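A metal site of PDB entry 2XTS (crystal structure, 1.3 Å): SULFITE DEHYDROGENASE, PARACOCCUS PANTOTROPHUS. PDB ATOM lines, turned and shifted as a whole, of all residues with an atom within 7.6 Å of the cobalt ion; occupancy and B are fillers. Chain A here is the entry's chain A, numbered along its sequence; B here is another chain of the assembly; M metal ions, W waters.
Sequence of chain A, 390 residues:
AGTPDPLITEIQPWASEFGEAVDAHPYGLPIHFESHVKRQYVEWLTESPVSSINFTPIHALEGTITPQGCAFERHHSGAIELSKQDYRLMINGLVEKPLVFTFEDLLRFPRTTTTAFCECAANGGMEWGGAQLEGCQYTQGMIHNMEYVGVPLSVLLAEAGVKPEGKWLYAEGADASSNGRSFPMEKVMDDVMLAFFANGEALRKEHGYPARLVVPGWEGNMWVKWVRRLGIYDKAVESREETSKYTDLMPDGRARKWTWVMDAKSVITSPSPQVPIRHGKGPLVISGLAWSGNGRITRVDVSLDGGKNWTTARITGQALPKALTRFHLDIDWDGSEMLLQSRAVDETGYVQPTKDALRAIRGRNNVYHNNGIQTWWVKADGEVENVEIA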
ATOM      1  N   ALA A 121       8.903 -31.520 -24.028  1.00  0.00           N
ATOM      2  CA  ALA A 121       9.206 -30.933 -22.749  1.00  0.00           C
ATOM      3  C   ALA A 121      10.505 -31.472 -22.182  1.00  0.00           C
ATOM      4  O   ALA A 121      11.218 -30.759 -21.457  1.00  0.00           O
ATOM      5  CB  ALA A 121       8.079 -31.243 -21.766  1.00  0.00           C
ATOM      6  N   ARG A 181      -4.798 -33.869 -22.296  1.00  0.00           N
ATOM      7  CA  ARG A 181      -4.240 -32.655 -21.742  1.00  0.00           C
ATOM      8  C   ARG A 181      -5.293 -31.556 -21.698  1.00  0.00           C
ATOM      9  O   ARG A 181      -6.108 -31.426 -22.603  1.00  0.00           O
ATOM     10  CB  ARG A 181      -3.011 -32.161 -22.546  1.00  0.00           C
ATOM     11  CG  ARG A 181      -1.756 -32.988 -22.376  1.00  0.00           C
ATOM     12  CD  ARG A 181      -1.246 -32.995 -20.952  1.00  0.00           C
ATOM     13  NE  ARG A 181      -0.915 -31.700 -20.414  1.00  0.00           N
ATOM     14  CZ  ARG A 181       0.277 -31.109 -20.425  1.00  0.00           C
ATOM     15  NH1 ARG A 181       1.326 -31.675 -20.980  1.00  0.00           N
ATOM     16  NH2 ARG A 181       0.421 -29.940 -19.847  1.00  0.00           N
ATOM     17  N   GLU A 219       4.765 -26.926 -24.936  1.00  0.00           N
ATOM     18  CA  GLU A 219       5.458 -28.184 -24.848  1.00  0.00           C
ATOM     19  C   GLU A 219       4.816 -29.251 -25.698  1.00  0.00           C
ATOM     20  O   GLU A 219       3.592 -29.360 -25.803  1.00  0.00           O
ATOM     21  CB  GLU A 219       5.579 -28.604 -23.369  1.00  0.00           C
ATOM     22  CG  GLU A 219       4.258 -29.030 -22.715  1.00  0.00           C
ATOM     23  CD  GLU A 219       4.320 -29.158 -21.188  1.00  0.00           C
ATOM     24  OE1 GLU A 219       5.403 -28.927 -20.602  1.00  0.00           O
ATOM     25  OE2 GLU A 219       3.261 -29.478 -20.585  1.00  0.00           O
ATOM     26  N   MET A 222       1.530 -31.434 -25.428  1.00  0.00           N
ATOM     27  CA  MET A 222       0.199 -30.907 -25.635  1.00  0.00           C
ATOM     28  C   MET A 222      -0.235 -31.007 -27.093  1.00  0.00           C
ATOM     29  O   MET A 222      -1.404 -30.771 -27.389  1.00  0.00           O
ATOM     30  CB  MET A 222       0.141 -29.505 -25.089  1.00  0.00           C
ATOM     31  CG  MET A 222       0.471 -29.453 -23.613  1.00  0.00           C
ATOM     32  SD  MET A 222       0.392 -27.768 -22.962  1.00  0.00           S
ATOM     33  CE  MET A 222      -1.343 -27.615 -22.576  1.00  0.00           C
ATOM     34  N   LYS A 245       3.226 -36.620 -14.824  1.00  0.00           N
ATOM     35  CA  LYS A 245       4.190 -36.209 -15.836  1.00  0.00           C
ATOM     36  C   LYS A 245       3.933 -34.755 -16.210  1.00  0.00           C
ATOM     37  O   LYS A 245       2.865 -34.196 -15.926  1.00  0.00           O
ATOM     38  CB  LYS A 245       4.083 -37.136 -17.029  1.00  0.00           C
ATOM     39  CG  LYS A 245       4.256 -38.603 -16.646  1.00  0.00           C
ATOM     40  CD  LYS A 245       5.647 -38.932 -16.084  1.00  0.00           C
ATOM     41  CE  LYS A 245       5.780 -40.422 -15.875  1.00  0.00           C
ATOM     42  NZ  LYS A 245       7.141 -40.804 -15.484  1.00  0.00           N
ATOM     43  N   TYR A 246       4.940 -34.132 -16.804  1.00  0.00           N
ATOM     44  CA  TYR A 246       4.919 -32.736 -17.248  1.00  0.00           C
ATOM     45  C   TYR A 246       4.558 -31.806 -16.082  1.00  0.00           C
ATOM     46  O   TYR A 246       3.905 -30.776 -16.235  1.00  0.00           O
ATOM     47  CB  TYR A 246       4.087 -32.531 -18.538  1.00  0.00           C
ATOM     48  CG  TYR A 246       4.498 -33.568 -19.543  1.00  0.00           C
ATOM     49  CD1 TYR A 246       5.699 -33.485 -20.213  1.00  0.00           C
ATOM     50  CD2 TYR A 246       3.734 -34.715 -19.720  1.00  0.00           C
ATOM     51  CE1 TYR A 246       6.102 -34.502 -21.097  1.00  0.00           C
ATOM     52  CE2 TYR A 246       4.137 -35.732 -20.562  1.00  0.00           C
ATOM     53  CZ  TYR A 246       5.308 -35.641 -21.236  1.00  0.00           C
ATOM     54  OH  TYR A 246       5.668 -36.709 -22.016  1.00  0.00           O
ATOM     55  N   THR A 247       5.090 -32.169 -14.922  1.00  0.00           N
ATOM     56  CA  THR A 247       5.164 -31.327 -13.739  1.00  0.00           C
ATOM     57  C   THR A 247       6.608 -31.345 -13.313  1.00  0.00           C
ATOM     58  O   THR A 247       7.312 -32.343 -13.511  1.00  0.00           O
ATOM     59  CB  THR A 247       4.269 -31.834 -12.600  1.00  0.00           C
ATOM     60  OG1 THR A 247       4.587 -33.214 -12.331  1.00  0.00           O
ATOM     61  CG2 THR A 247       2.797 -31.728 -12.976  1.00  0.00           C
ATOM     62  N   ASP A 248       7.084 -30.253 -12.726  1.00  0.00           N
ATOM     63  CA  ASP A 248       8.516 -29.948 -12.680  1.00  0.00           C
ATOM     64  C   ASP A 248       8.920 -29.763 -11.204  1.00  0.00           C
ATOM     65  O   ASP A 248       8.630 -28.718 -10.585  1.00  0.00           O
ATOM     66  CB  ASP A 248       8.820 -28.675 -13.469  1.00  0.00           C
ATOM     67  CG  ASP A 248       8.158 -28.630 -14.830  1.00  0.00           C
ATOM     68  OD1 ASP A 248       7.804 -29.688 -15.371  1.00  0.00           O
ATOM     69  OD2 ASP A 248       8.003 -27.482 -15.341  1.00  0.00           O
ATOM     70  N   ARG A 256       6.113 -27.329  -9.994  1.00  0.00           N
ATOM     71  CA  ARG A 256       5.326 -26.536 -10.921  1.00  0.00           C
ATOM     72  C   ARG A 256       4.434 -27.438 -11.758  1.00  0.00           C
ATOM     73  O   ARG A 256       4.900 -28.473 -12.251  1.00  0.00           O
ATOM     74  CB  ARG A 256       6.213 -25.710 -11.845  1.00  0.00           C
ATOM     75  CG  ARG A 256       7.041 -24.659 -11.172  1.00  0.00           C
ATOM     76  CD  ARG A 256       8.035 -24.069 -12.138  1.00  0.00           C
ATOM     77  NE  ARG A 256       8.779 -22.940 -11.610  1.00  0.00           N
ATOM     78  CZ  ARG A 256       9.897 -22.484 -12.152  1.00  0.00           C
ATOM     79  NH1 ARG A 256      10.419 -23.089 -13.214  1.00  0.00           N
ATOM     80  NH2 ARG A 256      10.517 -21.416 -11.646  1.00  0.00           N
ATOM     81  N   LYS A 257       3.185 -27.002 -11.940  1.00  0.00           N
ATOM     82  CA  LYS A 257       2.321 -27.637 -12.919  1.00  0.00           C
ATOM     83  C   LYS A 257       2.010 -26.611 -14.007  1.00  0.00           C
ATOM     84  O   LYS A 257       2.216 -25.416 -13.831  1.00  0.00           O
ATOM     85  CB  LYS A 257       1.024 -28.178 -12.291  1.00  0.00           C
ATOM     86  CG  LYS A 257       0.089 -27.099 -11.740  1.00  0.00           C
ATOM     87  CD  LYS A 257      -1.206 -27.691 -11.199  1.00  0.00           C
ATOM     88  CE  LYS A 257      -2.172 -26.638 -10.683  1.00  0.00           C
ATOM     89  NZ  LYS A 257      -3.367 -27.331 -10.149  1.00  0.00           N
ATOM     90  N   TRP A 258       1.511 -27.104 -15.132  1.00  0.00           N
ATOM     91  CA  TRP A 258       0.991 -26.264 -16.200  1.00  0.00           C
ATOM     92  C   TRP A 258       2.132 -25.371 -16.690  1.00  0.00           C
ATOM     93  O   TRP A 258       1.922 -24.204 -16.973  1.00  0.00           O
ATOM     94  CB  TRP A 258      -0.207 -25.444 -15.734  1.00  0.00           C
ATOM     95  CG  TRP A 258      -1.380 -26.210 -15.227  1.00  0.00           C
ATOM     96  CD1 TRP A 258      -1.615 -27.563 -15.282  1.00  0.00           C
ATOM     97  CD2 TRP A 258      -2.466 -25.635 -14.519  1.00  0.00           C
ATOM     98  NE1 TRP A 258      -2.815 -27.843 -14.656  1.00  0.00           N
ATOM     99  CE2 TRP A 258      -3.356 -26.677 -14.185  1.00  0.00           C
ATOM    100  CE3 TRP A 258      -2.786 -24.323 -14.150  1.00  0.00           C
ATOM    101  CZ2 TRP A 258      -4.546 -26.427 -13.473  1.00  0.00           C
ATOM    102  CZ3 TRP A 258      -3.969 -24.087 -13.462  1.00  0.00           C
ATOM    103  CH2 TRP A 258      -4.827 -25.134 -13.133  1.00  0.00           C
ATOM    104  N   THR A 259       3.361 -25.926 -16.831  1.00  0.00           N
ATOM    105  CA  THR A 259       4.458 -25.196 -17.439  1.00  0.00           C
ATOM    106  C   THR A 259       4.306 -25.453 -18.922  1.00  0.00           C
ATOM    107  O   THR A 259       4.899 -26.368 -19.503  1.00  0.00           O
ATOM    108  CB  THR A 259       5.822 -25.633 -16.871  1.00  0.00           C
ATOM    109  OG1 THR A 259       5.919 -27.075 -16.869  1.00  0.00           O
ATOM    110  CG2 THR A 259       5.929 -25.130 -15.436  1.00  0.00           C
ATOM    111  N   TRP A 260       3.466 -24.663 -19.532  1.00  0.00           N
ATOM    112  CA  TRP A 260       3.082 -24.891 -20.909  1.00  0.00           C
ATOM    113  C   TRP A 260       4.124 -24.364 -21.893  1.00  0.00           C
ATOM    114  O   TRP A 260       4.475 -25.043 -22.865  1.00  0.00           O
ATOM    115  CB  TRP A 260       1.720 -24.257 -21.189  1.00  0.00           C
ATOM    116  CG  TRP A 260       0.621 -24.828 -20.346  1.00  0.00           C
ATOM    117  CD1 TRP A 260       0.390 -26.137 -20.081  1.00  0.00           C
ATOM    118  CD2 TRP A 260      -0.438 -24.098 -19.705  1.00  0.00           C
ATOM    119  NE1 TRP A 260      -0.726 -26.265 -19.278  1.00  0.00           N
ATOM    120  CE2 TRP A 260      -1.258 -25.028 -19.039  1.00  0.00           C
ATOM    121  CE3 TRP A 260      -0.731 -22.739 -19.593  1.00  0.00           C
ATOM    122  CZ2 TRP A 260      -2.381 -24.643 -18.297  1.00  0.00           C
ATOM    123  CZ3 TRP A 260      -1.845 -22.366 -18.842  1.00  0.00           C
ATOM    124  CH2 TRP A 260      -2.647 -23.307 -18.206  1.00  0.00           C
ATOM    125  N   VAL A 261       4.595 -23.138 -21.716  1.00  0.00           N
ATOM    126  CA  VAL A 261       5.452 -22.512 -22.723  1.00  0.00           C
ATOM    127  C   VAL A 261       6.877 -23.035 -22.654  1.00  0.00           C
ATOM    128  O   VAL A 261       7.417 -23.353 -21.586  1.00  0.00           O
ATOM    129  CB  VAL A 261       5.434 -20.953 -22.740  1.00  0.00           C
ATOM    130  CG1 VAL A 261       5.819 -20.412 -24.128  1.00  0.00           C
ATOM    131  CG2 VAL A 261       4.091 -20.394 -22.421  1.00  0.00           C
ATOM    132  N   MET A 262       7.471 -23.153 -23.841  1.00  0.00           N
ATOM    133  CA  MET A 262       8.869 -23.493 -24.013  1.00  0.00           C
ATOM    134  C   MET A 262       9.674 -22.181 -24.141  1.00  0.00           C
ATOM    135  O   MET A 262       9.407 -21.361 -25.011  1.00  0.00           O
ATOM    136  CB  MET A 262       9.056 -24.387 -25.238  1.00  0.00           C
ATOM    137  CG  MET A 262       8.259 -25.676 -25.197  1.00  0.00           C
ATOM    138  SD  MET A 262       8.668 -26.722 -23.776  1.00  0.00           S
ATOM    139  CE  MET A 262      10.247 -27.404 -24.279  1.00  0.00           C
ATOM    140  N   TYR A 368      12.095 -31.514 -16.970  1.00  0.00           N
ATOM    141  CA  TYR A 368      11.598 -30.876 -18.173  1.00  0.00           C
ATOM    142  C   TYR A 368      12.195 -29.461 -18.276  1.00  0.00           C
ATOM    143  O   TYR A 368      12.816 -28.940 -17.328  1.00  0.00           O
ATOM    144  CB  TYR A 368      10.075 -30.806 -18.103  1.00  0.00           C
ATOM    145  CG  TYR A 368       9.407 -32.153 -17.891  1.00  0.00           C
ATOM    146  CD1 TYR A 368       9.345 -33.083 -18.926  1.00  0.00           C
ATOM    147  CD2 TYR A 368       8.855 -32.504 -16.677  1.00  0.00           C
ATOM    148  CE1 TYR A 368       8.743 -34.317 -18.763  1.00  0.00           C
ATOM    149  CE2 TYR A 368       8.282 -33.748 -16.500  1.00  0.00           C
ATOM    150  CZ  TYR A 368       8.219 -34.647 -17.537  1.00  0.00           C
ATOM    151  OH  TYR A 368       7.557 -35.843 -17.346  1.00  0.00           O
ATOM    152  N   HIS A 369      11.960 -28.807 -19.418  1.00  0.00           N
ATOM    153  CA  HIS A 369      12.244 -27.391 -19.589  1.00  0.00           C
ATOM    154  C   HIS A 369      13.706 -26.999 -19.384  1.00  0.00           C
ATOM    155  O   HIS A 369      14.005 -25.929 -18.874  1.00  0.00           O
ATOM    156  CB  HIS A 369      11.298 -26.529 -18.760  1.00  0.00           C
ATOM    157  CG  HIS A 369       9.864 -26.710 -19.133  1.00  0.00           C
ATOM    158  ND1 HIS A 369       9.298 -26.123 -20.249  1.00  0.00           N
ATOM    159  CD2 HIS A 369       8.862 -27.415 -18.539  1.00  0.00           C
ATOM    160  CE1 HIS A 369       8.026 -26.500 -20.344  1.00  0.00           C
ATOM    161  NE2 HIS A 369       7.737 -27.273 -19.306  1.00  0.00           N
ATOM    162  N   ASP B 149       2.639 -22.667 -13.008  1.00  0.00           N
ATOM    163  CA  ASP B 149       3.843 -22.052 -13.561  1.00  0.00           C
ATOM    164  C   ASP B 149       3.979 -20.603 -13.108  1.00  0.00           C
ATOM    165  O   ASP B 149       3.109 -19.775 -13.386  1.00  0.00           O
ATOM    166  CB  ASP B 149       3.721 -22.107 -15.088  1.00  0.00           C
ATOM    167  CG  ASP B 149       4.960 -21.657 -15.838  1.00  0.00           C
ATOM    168  OD1 ASP B 149       5.992 -21.322 -15.235  1.00  0.00           O
ATOM    169  OD2 ASP B 149       4.870 -21.623 -17.089  1.00  0.00           O
ATOM    170  N   ARG B 151       7.190 -18.991 -13.659  1.00  0.00           N
ATOM    171  CA  ARG B 151       8.382 -18.466 -14.314  1.00  0.00           C
ATOM    172  C   ARG B 151       8.258 -16.976 -14.563  1.00  0.00           C
ATOM    173  O   ARG B 151       9.260 -16.270 -14.499  1.00  0.00           O
ATOM    174  CB  ARG B 151       8.618 -19.189 -15.619  1.00  0.00           C
ATOM    175  CG  ARG B 151       9.208 -20.552 -15.413  1.00  0.00           C
ATOM    176  CD  ARG B 151       9.398 -21.284 -16.741  1.00  0.00           C
ATOM    177  NE  ARG B 151       8.121 -21.749 -17.275  1.00  0.00           N
ATOM    178  CZ  ARG B 151       7.960 -22.344 -18.452  1.00  0.00           C
ATOM    179  NH1 ARG B 151       9.017 -22.531 -19.228  1.00  0.00           N
ATOM    180  NH2 ARG B 151       6.754 -22.780 -18.814  1.00  0.00           N
HETATM  181 CO    CO M   1       5.825 -28.097 -18.753  1.00  0.00          CO
HETATM  182  O   HOH W   1       6.740 -29.755 -17.795  1.00  0.00           O
HETATM  183  O   HOH W   2       3.880 -28.741 -18.104  1.00  0.00           O
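The nearest printed residue that does not touch the cobalt ion is Asp 248 (4.1 Å).
The backbone NH (N) of Glu 219 is in hydrogen-bond range of the backbone carbonyl oxygen (O) of Trp 260. OE2 of Glu 219 lies within salt-bridge range of NH1 of Arg 181 (3.0 Å). OG1 of Thr 259 sits close to OD2 of Asp 248. O of Ala 121 lies within hydrogen-bond range of N of His 369, 2.9 Å away. A ring nitrogen (ND1) of His 369 lies close to the side-chain sulfur (SD) of Met 262, at 3.6 Å.
Water W2 lies within hydrogen-bond range of the side-chain carboxylate of Glu 219 (2.7 Å), the backbone carbonyl oxygen of Tyr 246 (2.8 Å) and the backbone NH of Thr 259 (3.1 Å). Water W1 lies within hydrogen-bond range of the side-chain carboxylate of Asp 248 (2.6 Å) and the backbone carbonyl oxygen of Tyr 246 (3.4 Å).
OE1 of Glu 219 is bound to the cobalt ion. O of Thr 259 binds the cobalt ion (2.1 Å). The cobalt ion is bound by water W1. OG1 of Thr 259 binds the cobalt ion (2.1 Å). Water W2 is bound to the cobalt ion, at 2.1 Å. The cobalt ion is bound by NE2 of His 369 (2.2 Å).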
